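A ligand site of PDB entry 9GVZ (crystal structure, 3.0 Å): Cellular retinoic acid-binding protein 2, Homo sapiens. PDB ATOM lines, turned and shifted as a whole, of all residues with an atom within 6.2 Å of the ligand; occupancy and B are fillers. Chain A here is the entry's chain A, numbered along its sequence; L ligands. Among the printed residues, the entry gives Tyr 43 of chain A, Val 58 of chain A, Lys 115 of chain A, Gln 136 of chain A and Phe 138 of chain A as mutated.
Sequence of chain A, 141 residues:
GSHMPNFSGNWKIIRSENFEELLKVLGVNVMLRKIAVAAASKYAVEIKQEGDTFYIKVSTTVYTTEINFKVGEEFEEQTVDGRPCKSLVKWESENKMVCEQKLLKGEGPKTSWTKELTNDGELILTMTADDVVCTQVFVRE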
ATOM      1  N   PHE A  19      26.417  28.828  19.826  1.00  0.00           N
ATOM      2  CA  PHE A  19      27.107  28.525  21.066  1.00  0.00           C
ATOM      3  C   PHE A  19      28.253  29.520  21.273  1.00  0.00           C
ATOM      4  O   PHE A  19      28.482  29.996  22.378  1.00  0.00           O
ATOM      5  CB  PHE A  19      27.466  27.036  21.117  1.00  0.00           C
ATOM      6  CG  PHE A  19      28.110  26.560  22.396  1.00  0.00           C
ATOM      7  CD1 PHE A  19      27.596  26.914  23.630  1.00  0.00           C
ATOM      8  CD2 PHE A  19      29.235  25.764  22.356  1.00  0.00           C
ATOM      9  CE1 PHE A  19      28.198  26.486  24.800  1.00  0.00           C
ATOM     10  CE2 PHE A  19      29.839  25.335  23.539  1.00  0.00           C
ATOM     11  CZ  PHE A  19      29.323  25.691  24.760  1.00  0.00           C
ATOM     12  N   ALA A  40      31.620  20.694  21.966  1.00  0.00           N
ATOM     13  CA  ALA A  40      30.191  20.735  22.193  1.00  0.00           C
ATOM     14  C   ALA A  40      29.423  19.858  21.203  1.00  0.00           C
ATOM     15  O   ALA A  40      28.198  19.868  21.185  1.00  0.00           O
ATOM     16  CB  ALA A  40      29.711  22.159  22.085  1.00  0.00           C
ATOM     17  N   TYR A  43      28.188  16.724  23.475  1.00  0.00           N
ATOM     18  CA  TYR A  43      27.269  16.918  24.602  1.00  0.00           C
ATOM     19  C   TYR A  43      26.288  15.755  24.706  1.00  0.00           C
ATOM     20  O   TYR A  43      25.591  15.435  23.737  1.00  0.00           O
ATOM     21  CB  TYR A  43      26.451  18.210  24.517  1.00  0.00           C
ATOM     22  CG  TYR A  43      27.158  19.420  25.082  1.00  0.00           C
ATOM     23  CD1 TYR A  43      27.690  19.392  26.364  1.00  0.00           C
ATOM     24  CD2 TYR A  43      27.338  20.560  24.334  1.00  0.00           C
ATOM     25  CE1 TYR A  43      28.379  20.485  26.885  1.00  0.00           C
ATOM     26  CE2 TYR A  43      28.023  21.657  24.828  1.00  0.00           C
ATOM     27  CZ  TYR A  43      28.547  21.614  26.109  1.00  0.00           C
ATOM     28  OH  TYR A  43      29.219  22.690  26.608  1.00  0.00           O
ATOM     29  N   VAL A  45      23.185  14.540  27.497  1.00  0.00           N
ATOM     30  CA  VAL A  45      22.347  14.880  28.634  1.00  0.00           C
ATOM     31  C   VAL A  45      21.552  13.632  28.995  1.00  0.00           C
ATOM     32  O   VAL A  45      20.770  13.135  28.185  1.00  0.00           O
ATOM     33  CB  VAL A  45      21.422  16.056  28.295  1.00  0.00           C
ATOM     34  CG1 VAL A  45      20.460  16.373  29.440  1.00  0.00           C
ATOM     35  CG2 VAL A  45      22.201  17.301  27.908  1.00  0.00           C
ATOM     36  N   ILE A  56      19.853  15.858  36.232  1.00  0.00           N
ATOM     37  CA  ILE A  56      20.409  16.043  34.919  1.00  0.00           C
ATOM     38  C   ILE A  56      21.929  15.930  34.971  1.00  0.00           C
ATOM     39  O   ILE A  56      22.574  16.730  35.651  1.00  0.00           O
ATOM     40  CB  ILE A  56      19.923  17.355  34.275  1.00  0.00           C
ATOM     41  CG1 ILE A  56      18.395  17.426  34.232  1.00  0.00           C
ATOM     42  CG2 ILE A  56      20.526  17.504  32.877  1.00  0.00           C
ATOM     43  CD1 ILE A  56      17.846  18.810  33.983  1.00  0.00           C
ATOM     44  N   VAL A  58      25.168  16.119  32.521  1.00  0.00           N
ATOM     45  CA  VAL A  58      25.582  16.798  31.303  1.00  0.00           C
ATOM     46  C   VAL A  58      27.085  16.575  31.139  1.00  0.00           C
ATOM     47  O   VAL A  58      27.903  17.076  31.907  1.00  0.00           O
ATOM     48  CB  VAL A  58      25.242  18.293  31.321  1.00  0.00           C
ATOM     49  CG1 VAL A  58      25.723  18.994  30.067  1.00  0.00           C
ATOM     50  CG2 VAL A  58      23.753  18.486  31.449  1.00  0.00           C
ATOM     51  N   THR A  65      28.772  17.090  34.475  1.00  0.00           N
ATOM     52  CA  THR A  65      28.165  17.595  35.695  1.00  0.00           C
ATOM     53  C   THR A  65      26.746  17.092  35.883  1.00  0.00           C
ATOM     54  O   THR A  65      26.021  16.836  34.920  1.00  0.00           O
ATOM     55  CB  THR A  65      28.301  19.117  35.914  1.00  0.00           C
ATOM     56  OG1 THR A  65      28.506  19.716  34.649  1.00  0.00           O
ATOM     57  CG2 THR A  65      29.411  19.467  36.876  1.00  0.00           C
ATOM     58  N   ILE A  67      23.357  18.208  37.905  1.00  0.00           N
ATOM     59  CA  ILE A  67      22.587  19.140  38.700  1.00  0.00           C
ATOM     60  C   ILE A  67      21.308  18.433  39.148  1.00  0.00           C
ATOM     61  O   ILE A  67      20.790  17.539  38.472  1.00  0.00           O
ATOM     62  CB  ILE A  67      22.335  20.456  37.935  1.00  0.00           C
ATOM     63  CG1 ILE A  67      20.878  20.665  37.562  1.00  0.00           C
ATOM     64  CG2 ILE A  67      23.226  20.560  36.711  1.00  0.00           C
ATOM     65  CD1 ILE A  67      20.599  22.062  37.087  1.00  0.00           C
ATOM     66  N   GLU A  77      23.928  26.270  41.041  1.00  0.00           N
ATOM     67  CA  GLU A  77      24.593  25.619  39.935  1.00  0.00           C
ATOM     68  C   GLU A  77      25.680  26.560  39.428  1.00  0.00           C
ATOM     69  O   GLU A  77      26.055  27.497  40.139  1.00  0.00           O
ATOM     70  CB  GLU A  77      23.598  25.137  38.864  1.00  0.00           C
ATOM     71  CG  GLU A  77      22.838  26.248  38.137  1.00  0.00           C
ATOM     72  CD  GLU A  77      22.074  25.894  36.855  1.00  0.00           C
ATOM     73  OE1 GLU A  77      22.256  24.780  36.316  1.00  0.00           O
ATOM     74  OE2 GLU A  77      21.307  26.757  36.382  1.00  0.00           O
ATOM     75  N   GLN A  78      26.202  26.283  38.232  1.00  0.00           N
ATOM     76  CA  GLN A  78      27.110  27.224  37.600  1.00  0.00           C
ATOM     77  C   GLN A  78      26.515  27.649  36.256  1.00  0.00           C
ATOM     78  O   GLN A  78      25.736  26.909  35.656  1.00  0.00           O
ATOM     79  CB  GLN A  78      28.532  26.647  37.519  1.00  0.00           C
ATOM     80  CG  GLN A  78      28.725  25.581  36.444  1.00  0.00           C
ATOM     81  N   THR A  79      27.004  28.792  35.781  1.00  0.00           N
ATOM     82  CA  THR A  79      26.604  29.261  34.450  1.00  0.00           C
ATOM     83  C   THR A  79      27.235  28.331  33.424  1.00  0.00           C
ATOM     84  O   THR A  79      27.688  27.235  33.808  1.00  0.00           O
ATOM     85  CB  THR A  79      27.152  30.660  34.214  1.00  0.00           C
ATOM     86  OG1 THR A  79      28.568  30.543  34.137  1.00  0.00           O
ATOM     87  CG2 THR A  79      26.784  31.623  35.321  1.00  0.00           C
ATOM     88  N   VAL A  80      27.283  28.748  32.171  1.00  0.00           N
ATOM     89  CA  VAL A  80      27.935  27.943  31.152  1.00  0.00           C
ATOM     90  C   VAL A  80      29.428  28.237  31.189  1.00  0.00           C
ATOM     91  O   VAL A  80      30.245  27.345  30.943  1.00  0.00           O
ATOM     92  CB  VAL A  80      27.376  28.207  29.736  1.00  0.00           C
ATOM     93  CG1 VAL A  80      27.500  26.980  28.842  1.00  0.00           C
ATOM     94  CG2 VAL A  80      25.951  28.725  29.765  1.00  0.00           C
ATOM     95  N   ASP A  81      29.766  29.508  31.464  1.00  0.00           N
ATOM     96  CA  ASP A  81      31.148  29.950  31.554  1.00  0.00           C
ATOM     97  C   ASP A  81      31.702  29.544  32.922  1.00  0.00           C
ATOM     98  O   ASP A  81      32.845  29.848  33.251  1.00  0.00           O
ATOM     99  CB  ASP A  81      31.311  31.422  31.148  1.00  0.00           C
ATOM    100  CG  ASP A  81      30.936  32.450  32.208  1.00  0.00           C
ATOM    101  OD1 ASP A  81      29.786  32.413  32.678  1.00  0.00           O
ATOM    102  OD2 ASP A  81      31.794  33.278  32.563  1.00  0.00           O
ATOM    103  N   GLY A  82      30.862  28.861  33.705  1.00  0.00           N
ATOM    104  CA  GLY A  82      31.263  28.235  34.954  1.00  0.00           C
ATOM    105  C   GLY A  82      31.461  29.247  36.078  1.00  0.00           C
ATOM    106  O   GLY A  82      32.487  29.235  36.747  1.00  0.00           O
ATOM    107  N   CYS A  99      14.700  28.525  33.482  1.00  0.00           N
ATOM    108  CA  CYS A  99      15.512  28.682  34.677  1.00  0.00           C
ATOM    109  C   CYS A  99      16.204  30.031  34.593  1.00  0.00           C
ATOM    110  O   CYS A  99      16.956  30.273  33.656  1.00  0.00           O
ATOM    111  CB  CYS A  99      16.594  27.611  34.726  1.00  0.00           C
ATOM    112  SG  CYS A  99      17.655  27.690  36.198  1.00  0.00           S
ATOM    113  N   GLN A 101      18.948  32.432  36.271  1.00  0.00           N
ATOM    114  CA  GLN A 101      20.144  32.369  37.110  1.00  0.00           C
ATOM    115  C   GLN A 101      20.495  33.768  37.567  1.00  0.00           C
ATOM    116  O   GLN A 101      20.450  34.725  36.783  1.00  0.00           O
ATOM    117  CB  GLN A 101      21.316  31.698  36.387  1.00  0.00           C
ATOM    118  CG  GLN A 101      20.912  30.431  35.632  1.00  0.00           C
ATOM    119  CD  GLN A 101      22.065  29.872  34.828  1.00  0.00           C
ATOM    120  OE1 GLN A 101      22.743  30.573  34.094  1.00  0.00           O
ATOM    121  NE2 GLN A 101      22.292  28.570  34.970  1.00  0.00           N
ATOM    122  N   SER A 112      20.190  32.645  31.349  1.00  0.00           N
ATOM    123  CA  SER A 112      19.066  31.754  31.602  1.00  0.00           C
ATOM    124  C   SER A 112      19.239  30.479  30.781  1.00  0.00           C
ATOM    125  O   SER A 112      20.138  30.370  29.951  1.00  0.00           O
ATOM    126  CB  SER A 112      17.785  32.418  31.234  1.00  0.00           C
ATOM    127  OG  SER A 112      17.590  32.282  29.841  1.00  0.00           O
ATOM    128  N   TRP A 113      18.346  29.520  31.018  1.00  0.00           N
ATOM    129  CA  TRP A 113      18.289  28.335  30.172  1.00  0.00           C
ATOM    130  C   TRP A 113      16.903  27.715  30.244  1.00  0.00           C
ATOM    131  O   TRP A 113      16.259  27.715  31.294  1.00  0.00           O
ATOM    132  CB  TRP A 113      19.380  27.314  30.531  1.00  0.00           C
ATOM    133  CG  TRP A 113      19.217  26.662  31.875  1.00  0.00           C
ATOM    134  CD1 TRP A 113      19.874  26.989  33.024  1.00  0.00           C
ATOM    135  CD2 TRP A 113      18.351  25.567  32.211  1.00  0.00           C
ATOM    136  NE1 TRP A 113      19.477  26.167  34.046  1.00  0.00           N
ATOM    137  CE2 TRP A 113      18.542  25.288  33.579  1.00  0.00           C
ATOM    138  CE3 TRP A 113      17.436  24.781  31.487  1.00  0.00           C
ATOM    139  CZ2 TRP A 113      17.855  24.274  34.240  1.00  0.00           C
ATOM    140  CZ3 TRP A 113      16.750  23.781  32.143  1.00  0.00           C
ATOM    141  CH2 TRP A 113      16.966  23.541  33.499  1.00  0.00           C
ATOM    142  N   THR A 114      16.491  27.157  29.111  1.00  0.00           N
ATOM    143  CA  THR A 114      15.244  26.420  29.058  1.00  0.00           C
ATOM    144  C   THR A 114      15.475  25.050  28.438  1.00  0.00           C
ATOM    145  O   THR A 114      16.354  24.874  27.595  1.00  0.00           O
ATOM    146  CB  THR A 114      14.178  27.201  28.285  1.00  0.00           C
ATOM    147  OG1 THR A 114      14.396  26.728  26.962  1.00  0.00           O
ATOM    148  CG2 THR A 114      14.358  28.700  28.357  1.00  0.00           C
ATOM    149  N   LYS A 115      14.663  24.088  28.880  1.00  0.00           N
ATOM    150  CA  LYS A 115      14.556  22.774  28.276  1.00  0.00           C
ATOM    151  C   LYS A 115      13.098  22.546  27.882  1.00  0.00           C
ATOM    152  O   LYS A 115      12.165  22.879  28.619  1.00  0.00           O
ATOM    153  CB  LYS A 115      15.120  21.704  29.218  1.00  0.00           C
ATOM    154  CG  LYS A 115      16.637  21.621  29.232  1.00  0.00           C
ATOM    155  CD  LYS A 115      17.195  20.580  30.187  1.00  0.00           C
ATOM    156  CE  LYS A 115      18.570  20.063  29.783  1.00  0.00           C
ATOM    157  NZ  LYS A 115      19.525  21.133  29.358  1.00  0.00           N
ATOM    158  N   LEU A 125      17.328  22.664  23.994  1.00  0.00           N
ATOM    159  CA  LEU A 125      17.899  23.520  25.011  1.00  0.00           C
ATOM    160  C   LEU A 125      18.192  24.878  24.394  1.00  0.00           C
ATOM    161  O   LEU A 125      18.834  24.956  23.349  1.00  0.00           O
ATOM    162  CB  LEU A 125      19.189  22.890  25.556  1.00  0.00           C
ATOM    163  CG  LEU A 125      20.026  23.819  26.435  1.00  0.00           C
ATOM    164  CD1 LEU A 125      19.591  23.738  27.883  1.00  0.00           C
ATOM    165  CD2 LEU A 125      21.495  23.500  26.299  1.00  0.00           C
ATOM    166  N   MET A 127      19.831  28.688  25.710  1.00  0.00           N
ATOM    167  CA  MET A 127      20.636  29.318  26.752  1.00  0.00           C
ATOM    168  C   MET A 127      20.893  30.768  26.357  1.00  0.00           C
ATOM    169  O   MET A 127      21.594  31.038  25.374  1.00  0.00           O
ATOM    170  CB  MET A 127      21.979  28.620  26.910  1.00  0.00           C
ATOM    171  CG  MET A 127      21.900  27.139  27.152  1.00  0.00           C
ATOM    172  SD  MET A 127      23.563  26.396  27.097  1.00  0.00           S
ATOM    173  CE  MET A 127      23.693  25.958  25.365  1.00  0.00           C
ATOM    174  N   CYS A 134      21.530  30.887  22.536  1.00  0.00           N
ATOM    175  CA  CYS A 134      22.051  29.670  21.939  1.00  0.00           C
ATOM    176  C   CYS A 134      21.016  28.551  21.979  1.00  0.00           C
ATOM    177  O   CYS A 134      20.378  28.304  23.006  1.00  0.00           O
ATOM    178  CB  CYS A 134      23.360  29.235  22.590  1.00  0.00           C
ATOM    179  SG  CYS A 134      23.817  27.532  22.184  1.00  0.00           S
ATOM    180  N   GLN A 136      20.321  24.400  21.253  1.00  0.00           N
ATOM    181  CA  GLN A 136      20.894  23.090  21.032  1.00  0.00           C
ATOM    182  C   GLN A 136      19.769  22.080  20.993  1.00  0.00           C
ATOM    183  O   GLN A 136      18.872  22.085  21.828  1.00  0.00           O
ATOM    184  CB  GLN A 136      21.955  22.786  22.093  1.00  0.00           C
ATOM    185  CG  GLN A 136      23.214  23.606  21.918  1.00  0.00           C
ATOM    186  CD  GLN A 136      24.238  23.294  22.976  1.00  0.00           C
ATOM    187  OE1 GLN A 136      23.904  22.968  24.112  1.00  0.00           O
ATOM    188  NE2 GLN A 136      25.506  23.394  22.613  1.00  0.00           N
ATOM    189  N   PHE A 138      18.769  18.049  20.944  1.00  0.00           N
ATOM    190  CA  PHE A 138      19.198  16.716  21.290  1.00  0.00           C
ATOM    191  C   PHE A 138      18.140  15.709  20.837  1.00  0.00           C
ATOM    192  O   PHE A 138      16.961  16.033  20.728  1.00  0.00           O
ATOM    193  CB  PHE A 138      19.403  16.587  22.801  1.00  0.00           C
ATOM    194  CG  PHE A 138      20.463  17.487  23.368  1.00  0.00           C
ATOM    195  CD1 PHE A 138      20.319  18.869  23.334  1.00  0.00           C
ATOM    196  CD2 PHE A 138      21.592  16.947  23.951  1.00  0.00           C
ATOM    197  CE1 PHE A 138      21.279  19.699  23.869  1.00  0.00           C
ATOM    198  CE2 PHE A 138      22.568  17.788  24.478  1.00  0.00           C
ATOM    199  CZ  PHE A 138      22.410  19.152  24.436  1.00  0.00           C
HETATM  200  C1  LIG L   1      22.517  25.596  31.853  1.00  0.00           C
HETATM  201  O1  LIG L   1      22.732  24.140  31.975  1.00  0.00           O
HETATM  202  C2  LIG L   1      21.600  23.458  31.804  1.00  0.00           C
HETATM  203  O2  LIG L   1      20.699  23.552  32.596  1.00  0.00           O
HETATM  204  C3  LIG L   1      21.482  22.537  30.573  1.00  0.00           C
HETATM  205  C4  LIG L   1      20.221  21.797  30.399  1.00  0.00           C
HETATM  206  C5  LIG L   1      22.524  22.315  29.460  1.00  0.00           C
HETATM  207  C6  LIG L   1      23.787  22.795  29.559  1.00  0.00           C
HETATM  208  C7  LIG L   1      24.353  22.941  30.876  1.00  0.00           C
HETATM  209  C8  LIG L   1      25.620  23.413  31.067  1.00  0.00           C
HETATM  210  O3  LIG L   1      26.203  23.594  32.322  1.00  0.00           O
HETATM  211  C9  LIG L   1      27.359  24.443  32.434  1.00  0.00           C
HETATM  212  C10 LIG L   1      24.515  23.025  28.408  1.00  0.00           C
HETATM  213  C11 LIG L   1      25.791  23.467  28.600  1.00  0.00           C
HETATM  214  O4  LIG L   1      26.568  23.737  27.549  1.00  0.00           O
HETATM  215  C12 LIG L   1      25.711  23.826  26.389  1.00  0.00           C
HETATM  216  C13 LIG L   1      26.329  23.647  29.905  1.00  0.00           C
HETATM  217  O5  LIG L   1      27.570  24.075  30.079  1.00  0.00           O
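The side-chain sulfur (SG) of Cys 134 lies close to the backbone NH (N) of Phe 19.
O of Leu 125 lies within hydrogen-bond range of N of Gln 136 (2.6 Å).
The side-chain hydroxyl (OG1) of Thr 79 is in hydrogen-bond range of the side-chain carboxylate (OD1) of Asp 81 (2.7 Å).
The backbone carbonyl oxygen of Trp 113 is in hydrogen-bond range of the backbone NH of Cys 99 (2.8 Å).
The indole nitrogen of Trp 113 sits at hydrogen-bond distance from the side-chain carboxylate of Glu 77 (3.0 Å).
The backbone NH (N) of Met 127 lies within hydrogen-bond range of the backbone carbonyl oxygen (O) of Cys 134.
The side-chain hydroxyl (OG1) of Thr 79 lies within hydrogen-bond range of the backbone NH (N) of Gly 82.
Residues that only touch the ligand: Phe 19 (3.97 Å), Thr 79 (3.1 Å), Val 80 (3.2 Å), Leu 125 (3.2 Å), Met 127 (3.1 Å) and Gln 136 (3.0 Å).
Hydrophobic or aromatic side chains that line the ligand: Phe 19, Tyr 43, Val 80, Trp 113, Leu 125 and Met 127.
Within 4 Å of the ligand: Phe 19, Tyr 43, Thr 79, Val 80, Trp 113, Lys 115, Leu 125, Met 127 and Gln 136.
NZ of Lys 115 is bonded to C4 of the ligand (1.4 Å).
The indole nitrogen of Trp 113 sits close to an oxygen (O2) of the ligand, 3.2 Å away.
The side-chain hydroxyl (OH) of Tyr 43 is in hydrogen-bond range of an oxygen (O4) of the ligand.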
